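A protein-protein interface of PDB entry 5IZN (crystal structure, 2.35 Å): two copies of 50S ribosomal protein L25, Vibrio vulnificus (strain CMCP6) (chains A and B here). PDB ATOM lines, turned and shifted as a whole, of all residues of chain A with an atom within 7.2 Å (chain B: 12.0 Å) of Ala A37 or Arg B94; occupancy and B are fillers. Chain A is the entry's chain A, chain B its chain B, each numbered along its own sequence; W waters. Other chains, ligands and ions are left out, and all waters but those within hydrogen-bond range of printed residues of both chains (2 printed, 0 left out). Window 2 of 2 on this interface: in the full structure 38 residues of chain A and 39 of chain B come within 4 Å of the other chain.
N of Val A32 lies within hydrogen-bond range of O of Val A40 (3.0 Å).
The backbone carbonyl oxygen (O) of Val A32 is in hydrogen-bond range of the guanidinium group (NH2) of Arg B94, at 3.4 Å.
The backbone carbonyl oxygen (O) of Lys A72 is in hydrogen-bond range of the backbone NH (N) of Ile B95.
O of Gly A34 sits at hydrogen-bond distance from NH1 of Arg B94 (2.9 Å).
N of Lys A74 is in hydrogen-bond range of O of Ile B93 (2.8 Å).
The backbone NH of Gln A76 lies within hydrogen-bond range of the backbone carbonyl oxygen of Asp B91 (3.0 Å).
NH2 of Arg B94 lies within hydrogen-bond range of O of Ala A38, at 2.8 Å.
The backbone NH of Arg B94 lies within hydrogen-bond range of the backbone carbonyl oxygen of Tyr A33, at 2.8 Å.
The backbone NH (N) of Tyr A33 lies within hydrogen-bond range of the backbone carbonyl oxygen (O) of Phe B92, 2.8 Å away.
Phe B92 touches Val A32.
Tyr A33 touches Asp B91 (CE1 to CB, 3.8 Å).
CA of Ile B93 touches O of Tyr A33, at 3.2 Å.
CA of Gly A34 touches CG1 of Ile B93, at 3.7 Å.
Ala A37 touches Arg B94 (O to NH1, 3.6 Å).
Val A40 touches Arg B94 (CG1 to NH2, 3.9 Å).
Lys A72 touches Arg B94 (O to CA, 3.8 Å).
CA of Val A73 touches O of Ile B93 (3.1 Å).
Ile B95 touches Lys A74.
CD of Gln A76 touches CG2 of Ile B93, 3.5 Å away.
Water W1 lies within hydrogen-bond range of O of Gln A76 (2.5 Å) and N of Asp B91 (2.9 Å).
Water W2 bridges O of Lys A72 (2.8 Å) and O of Ile B95 (2.9 Å).
Of the 6 printed residues of chain B, 5 touch a printed residue of chain A.
Of the 15 printed residues of chain A, 10 touch a printed residue of chain B.
Hydrophobic or aromatic side chains of chain A within 4 Å of the printed part of chain B: Tyr A33, Ala A37, Val A40 and Val A73.
Along chain A the printed residues that touch a printed residue of chain B span positions 32 to 76.
Among the printed residues, 21 pairs touch across the chains.
Among the printed residues, no Asp or Glu carboxylate lies within 4 Å of a Lys or Arg side-chain nitrogen of the other chain.
No position is printed for both chains.
Of the 21 pairs that touch across the chains among the printed residues, none has its exchanged pair printed and touching as well.
Printed residues of chain B within 4 Å of Ala A37: Arg B94.
Printed residues of chain A within 4 Å of Arg B94: Val A32 (3.4 Å), Tyr A33 (2.8 Å), Gly A34 (2.9 Å), Ala A37 (3.6 Å), Ala A38 (2.8 Å), Val A40 (3.9 Å) and Lys A72 (3.8 Å).
Gly A35 touches none of the printed residues of chain B.
No residue of chain B comes within 4 Å of Glu A36.
No residue of chain B comes within 4 Å of Pro A39.
Of the printed residues of chain B, Gln A76 touches Asp B91 (3.0 Å) and Ile B93 (3.5 Å).
Printed residues of chain B within 4 Å of Val A32: Phe B92 and Arg B94.
The nearest printed residue of chain B that does not touch Ala A37 is Phe B92 (9.1 Å).
The nearest printed residue of chain A that does not touch Arg B94 is Gly A35 (4.2 Å).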
ATOM      1  N   VAL A  32       9.487 -24.733  -5.027  1.00  0.00           N
ATOM      2  CA  VAL A  32      10.717 -25.033  -5.745  1.00  0.00           C
ATOM      3  C   VAL A  32      11.852 -25.297  -4.764  1.00  0.00           C
ATOM      4  O   VAL A  32      12.306 -24.392  -4.064  1.00  0.00           O
ATOM      5  CB  VAL A  32      11.115 -23.890  -6.694  1.00  0.00           C
ATOM      6  CG1 VAL A  32      12.431 -24.210  -7.385  1.00  0.00           C
ATOM      7  CG2 VAL A  32      10.015 -23.645  -7.716  1.00  0.00           C
ATOM      8  N   TYR A  33      12.297 -26.547  -4.713  1.00  0.00           N
ATOM      9  CA  TYR A  33      13.375 -26.947  -3.818  1.00  0.00           C
ATOM     10  C   TYR A  33      14.453 -27.693  -4.595  1.00  0.00           C
ATOM     11  O   TYR A  33      14.441 -27.710  -5.825  1.00  0.00           O
ATOM     12  CB  TYR A  33      12.836 -27.822  -2.683  1.00  0.00           C
ATOM     13  CG  TYR A  33      12.384 -29.198  -3.123  1.00  0.00           C
ATOM     14  CD1 TYR A  33      11.200 -29.370  -3.832  1.00  0.00           C
ATOM     15  CD2 TYR A  33      13.136 -30.328  -2.824  1.00  0.00           C
ATOM     16  CE1 TYR A  33      10.783 -30.626  -4.235  1.00  0.00           C
ATOM     17  CE2 TYR A  33      12.726 -31.587  -3.221  1.00  0.00           C
ATOM     18  CZ  TYR A  33      11.549 -31.731  -3.926  1.00  0.00           C
ATOM     19  OH  TYR A  33      11.139 -32.983  -4.324  1.00  0.00           O
ATOM     20  N   GLY A  34      15.384 -28.308  -3.876  1.00  0.00           N
ATOM     21  CA  GLY A  34      16.420 -29.101  -4.509  1.00  0.00           C
ATOM     22  C   GLY A  34      17.756 -28.393  -4.564  1.00  0.00           C
ATOM     23  O   GLY A  34      17.871 -27.231  -4.169  1.00  0.00           O
ATOM     24  N   GLY A  35      18.766 -29.094  -5.071  1.00  0.00           N
ATOM     25  CA  GLY A  35      20.119 -28.574  -5.082  1.00  0.00           C
ATOM     26  C   GLY A  35      20.594 -28.371  -3.659  1.00  0.00           C
ATOM     27  O   GLY A  35      20.413 -29.241  -2.808  1.00  0.00           O
ATOM     28  N   GLU A  36      21.196 -27.218  -3.396  1.00  0.00           N
ATOM     29  CA  GLU A  36      21.593 -26.861  -2.040  1.00  0.00           C
ATOM     30  C   GLU A  36      21.155 -25.434  -1.729  1.00  0.00           C
ATOM     31  O   GLU A  36      21.800 -24.725  -0.958  1.00  0.00           O
ATOM     32  CB  GLU A  36      23.105 -27.017  -1.855  1.00  0.00           C
ATOM     33  CG  GLU A  36      23.616 -28.450  -2.011  1.00  0.00           C
ATOM     34  CD  GLU A  36      23.290 -29.339  -0.819  1.00  0.00           C
ATOM     35  OE1 GLU A  36      24.235 -29.772  -0.128  1.00  0.00           O
ATOM     36  OE2 GLU A  36      22.096 -29.618  -0.577  1.00  0.00           O
ATOM     37  N   ALA A  37      20.049 -25.024  -2.340  1.00  0.00           N
ATOM     38  CA  ALA A  37      19.504 -23.689  -2.136  1.00  0.00           C
ATOM     39  C   ALA A  37      18.212 -23.744  -1.330  1.00  0.00           C
ATOM     40  O   ALA A  37      17.590 -24.799  -1.206  1.00  0.00           O
ATOM     41  CB  ALA A  37      19.265 -23.005  -3.472  1.00  0.00           C
ATOM     42  N   ALA A  38      17.812 -22.599  -0.787  1.00  0.00           N
ATOM     43  CA  ALA A  38      16.607 -22.510   0.026  1.00  0.00           C
ATOM     44  C   ALA A  38      15.353 -22.714  -0.819  1.00  0.00           C
ATOM     45  O   ALA A  38      15.298 -22.282  -1.970  1.00  0.00           O
ATOM     46  CB  ALA A  38      16.551 -21.168   0.741  1.00  0.00           C
ATOM     47  N   PRO A  39      14.338 -23.380  -0.248  1.00  0.00           N
ATOM     48  CA  PRO A  39      13.061 -23.565  -0.943  1.00  0.00           C
ATOM     49  C   PRO A  39      12.313 -22.246  -1.105  1.00  0.00           C
ATOM     50  O   PRO A  39      12.517 -21.327  -0.313  1.00  0.00           O
ATOM     51  CB  PRO A  39      12.298 -24.523  -0.025  1.00  0.00           C
ATOM     52  CG  PRO A  39      12.880 -24.286   1.323  1.00  0.00           C
ATOM     53  CD  PRO A  39      14.333 -23.999   1.088  1.00  0.00           C
ATOM     54  N   VAL A  40      11.462 -22.157  -2.122  1.00  0.00           N
ATOM     55  CA  VAL A  40      10.695 -20.943  -2.367  1.00  0.00           C
ATOM     56  C   VAL A  40       9.272 -21.270  -2.816  1.00  0.00           C
ATOM     57  O   VAL A  40       9.062 -22.081  -3.719  1.00  0.00           O
ATOM     58  CB  VAL A  40      11.385 -20.047  -3.423  1.00  0.00           C
ATOM     59  CG1 VAL A  40      11.820 -20.867  -4.632  1.00  0.00           C
ATOM     60  CG2 VAL A  40      10.476 -18.899  -3.836  1.00  0.00           C
ATOM     61  N   ILE A  66      11.565 -17.372 -12.222  1.00  0.00           N
ATOM     62  CA  ILE A  66      11.383 -16.918 -10.849  1.00  0.00           C
ATOM     63  C   ILE A  66      12.139 -15.618 -10.592  1.00  0.00           C
ATOM     64  O   ILE A  66      13.361 -15.619 -10.449  1.00  0.00           O
ATOM     65  CB  ILE A  66      11.854 -17.980  -9.837  1.00  0.00           C
ATOM     66  CG1 ILE A  66      11.213 -19.334 -10.146  1.00  0.00           C
ATOM     67  CG2 ILE A  66      11.537 -17.540  -8.416  1.00  0.00           C
ATOM     68  CD1 ILE A  66      11.662 -20.445  -9.222  1.00  0.00           C
ATOM     69  N   VAL A  71      14.884 -20.814 -14.082  1.00  0.00           N
ATOM     70  CA  VAL A  71      15.320 -21.921 -13.238  1.00  0.00           C
ATOM     71  C   VAL A  71      14.883 -23.260 -13.821  1.00  0.00           C
ATOM     72  O   VAL A  71      13.688 -23.526 -13.965  1.00  0.00           O
ATOM     73  CB  VAL A  71      14.771 -21.792 -11.806  1.00  0.00           C
ATOM     74  CG1 VAL A  71      15.280 -22.932 -10.941  1.00  0.00           C
ATOM     75  CG2 VAL A  71      15.159 -20.449 -11.207  1.00  0.00           C
ATOM     76  N   LYS A  72      15.856 -24.100 -14.158  1.00  0.00           N
ATOM     77  CA  LYS A  72      15.574 -25.417 -14.714  1.00  0.00           C
ATOM     78  C   LYS A  72      15.179 -26.393 -13.611  1.00  0.00           C
ATOM     79  O   LYS A  72      15.993 -26.737 -12.756  1.00  0.00           O
ATOM     80  CB  LYS A  72      16.786 -25.945 -15.482  1.00  0.00           C
ATOM     81  CG  LYS A  72      16.561 -27.286 -16.161  1.00  0.00           C
ATOM     82  CD  LYS A  72      17.803 -27.730 -16.918  1.00  0.00           C
ATOM     83  CE  LYS A  72      17.574 -29.054 -17.629  1.00  0.00           C
ATOM     84  NZ  LYS A  72      18.785 -29.502 -18.373  1.00  0.00           N
ATOM     85  N   VAL A  73      13.926 -26.833 -13.634  1.00  0.00           N
ATOM     86  CA  VAL A  73      13.422 -27.728 -12.599  1.00  0.00           C
ATOM     87  C   VAL A  73      12.813 -29.002 -13.172  1.00  0.00           C
ATOM     88  O   VAL A  73      12.653 -29.143 -14.386  1.00  0.00           O
ATOM     89  CB  VAL A  73      12.357 -27.040 -11.723  1.00  0.00           C
ATOM     90  CG1 VAL A  73      12.926 -25.788 -11.074  1.00  0.00           C
ATOM     91  CG2 VAL A  73      11.127 -26.711 -12.550  1.00  0.00           C
ATOM     92  N   LYS A  74      12.470 -29.923 -12.279  1.00  0.00           N
ATOM     93  CA  LYS A  74      11.862 -31.188 -12.661  1.00  0.00           C
ATOM     94  C   LYS A  74      10.712 -31.523 -11.718  1.00  0.00           C
ATOM     95  O   LYS A  74      10.915 -31.649 -10.511  1.00  0.00           O
ATOM     96  CB  LYS A  74      12.908 -32.304 -12.651  1.00  0.00           C
ATOM     97  CG  LYS A  74      12.368 -33.682 -12.989  1.00  0.00           C
ATOM     98  CD  LYS A  74      13.482 -34.718 -12.964  1.00  0.00           C
ATOM     99  CE  LYS A  74      12.960 -36.108 -13.288  1.00  0.00           C
ATOM    100  NZ  LYS A  74      14.049 -37.125 -13.269  1.00  0.00           N
ATOM    101  N   GLN A  76       8.009 -33.304  -9.454  1.00  0.00           N
ATOM    102  CA  GLN A  76       8.193 -34.468  -8.593  1.00  0.00           C
ATOM    103  C   GLN A  76       6.869 -35.086  -8.155  1.00  0.00           C
ATOM    104  O   GLN A  76       5.991 -34.393  -7.637  1.00  0.00           O
ATOM    105  CB  GLN A  76       9.017 -34.089  -7.359  1.00  0.00           C
ATOM    106  CG  GLN A  76      10.429 -33.613  -7.668  1.00  0.00           C
ATOM    107  CD  GLN A  76      11.320 -34.717  -8.203  1.00  0.00           C
ATOM    108  OE1 GLN A  76      11.321 -35.006  -9.400  1.00  0.00           O
ATOM    109  NE2 GLN A  76      12.089 -35.339  -7.316  1.00  0.00           N
ATOM    110  N   MET B  90       1.982 -28.692  -6.550  1.00  0.00           N
ATOM    111  CA  MET B  90       3.042 -29.391  -7.265  1.00  0.00           C
ATOM    112  C   MET B  90       4.422 -29.001  -6.742  1.00  0.00           C
ATOM    113  O   MET B  90       4.683 -27.833  -6.456  1.00  0.00           O
ATOM    114  CB  MET B  90       2.944 -29.111  -8.766  1.00  0.00           C
ATOM    115  CG  MET B  90       3.859 -29.972  -9.621  1.00  0.00           C
ATOM    116  SD  MET B  90       3.425 -29.873 -11.519  1.00  0.00           S
ATOM    117  CE  MET B  90       1.603 -30.561 -11.455  1.00  0.00           C
ATOM    118  N   ASP B  91       5.301 -29.990  -6.611  1.00  0.00           N
ATOM    119  CA  ASP B  91       6.670 -29.755  -6.162  1.00  0.00           C
ATOM    120  C   ASP B  91       7.645 -29.789  -7.333  1.00  0.00           C
ATOM    121  O   ASP B  91       7.509 -30.607  -8.243  1.00  0.00           O
ATOM    122  CB  ASP B  91       7.079 -30.790  -5.112  1.00  0.00           C
ATOM    123  CG  ASP B  91       6.306 -30.644  -3.817  1.00  0.00           C
ATOM    124  OD1 ASP B  91       6.095 -29.495  -3.376  1.00  0.00           O
ATOM    125  OD2 ASP B  91       5.908 -31.678  -3.241  1.00  0.00           O
ATOM    126  N   PHE B  92       8.629 -28.897  -7.304  1.00  0.00           N
ATOM    127  CA  PHE B  92       9.632 -28.836  -8.360  1.00  0.00           C
ATOM    128  C   PHE B  92      11.038 -28.898  -7.781  1.00  0.00           C
ATOM    129  O   PHE B  92      11.358 -28.186  -6.829  1.00  0.00           O
ATOM    130  CB  PHE B  92       9.463 -27.565  -9.192  1.00  0.00           C
ATOM    131  CG  PHE B  92       8.132 -27.464  -9.876  1.00  0.00           C
ATOM    132  CD1 PHE B  92       7.954 -27.971 -11.153  1.00  0.00           C
ATOM    133  CD2 PHE B  92       7.057 -26.865  -9.242  1.00  0.00           C
ATOM    134  CE1 PHE B  92       6.730 -27.879 -11.785  1.00  0.00           C
ATOM    135  CE2 PHE B  92       5.830 -26.772  -9.869  1.00  0.00           C
ATOM    136  CZ  PHE B  92       5.668 -27.278 -11.142  1.00  0.00           C
ATOM    137  N   ILE B  93      11.875 -29.748  -8.362  1.00  0.00           N
ATOM    138  CA  ILE B  93      13.233 -29.925  -7.871  1.00  0.00           C
ATOM    139  C   ILE B  93      14.239 -29.343  -8.867  1.00  0.00           C
ATOM    140  O   ILE B  93      14.083 -29.484 -10.079  1.00  0.00           O
ATOM    141  CB  ILE B  93      13.531 -31.420  -7.589  1.00  0.00           C
ATOM    142  CG1 ILE B  93      14.744 -31.573  -6.674  1.00  0.00           C
ATOM    143  CG2 ILE B  93      13.708 -32.218  -8.878  1.00  0.00           C
ATOM    144  CD1 ILE B  93      14.943 -32.986  -6.208  1.00  0.00           C
ATOM    145  N   ARG B  94      15.255 -28.661  -8.349  1.00  0.00           N
ATOM    146  CA  ARG B  94      16.270 -28.046  -9.196  1.00  0.00           C
ATOM    147  C   ARG B  94      17.203 -29.099  -9.784  1.00  0.00           C
ATOM    148  O   ARG B  94      17.764 -29.918  -9.058  1.00  0.00           O
ATOM    149  CB  ARG B  94      17.076 -27.012  -8.408  1.00  0.00           C
ATOM    150  CG  ARG B  94      16.249 -25.866  -7.850  1.00  0.00           C
ATOM    151  CD  ARG B  94      17.129 -24.862  -7.121  1.00  0.00           C
ATOM    152  NE  ARG B  94      16.348 -23.807  -6.481  1.00  0.00           N
ATOM    153  CZ  ARG B  94      15.913 -23.855  -5.226  1.00  0.00           C
ATOM    154  NH1 ARG B  94      16.184 -24.911  -4.469  1.00  0.00           N
ATOM    155  NH2 ARG B  94      15.208 -22.849  -4.727  1.00  0.00           N
ATOM    156  N   ILE B  95      17.364 -29.071 -11.103  1.00  0.00           N
ATOM    157  CA  ILE B  95      18.231 -30.023 -11.786  1.00  0.00           C
ATOM    158  C   ILE B  95      19.285 -29.312 -12.629  1.00  0.00           C
ATOM    159  O   ILE B  95      19.168 -28.120 -12.909  1.00  0.00           O
ATOM    160  CB  ILE B  95      17.424 -30.973 -12.688  1.00  0.00           C
ATOM    161  CG1 ILE B  95      16.650 -30.175 -13.739  1.00  0.00           C
ATOM    162  CG2 ILE B  95      16.477 -31.821 -11.854  1.00  0.00           C
ATOM    163  CD1 ILE B  95      15.862 -31.038 -14.700  1.00  0.00           C
HETATM  164  O   HOH W   1       4.349 -32.662  -6.937  1.00  0.00           O
HETATM  165  O   HOH W   2      18.341 -25.749 -11.552  1.00  0.00           O
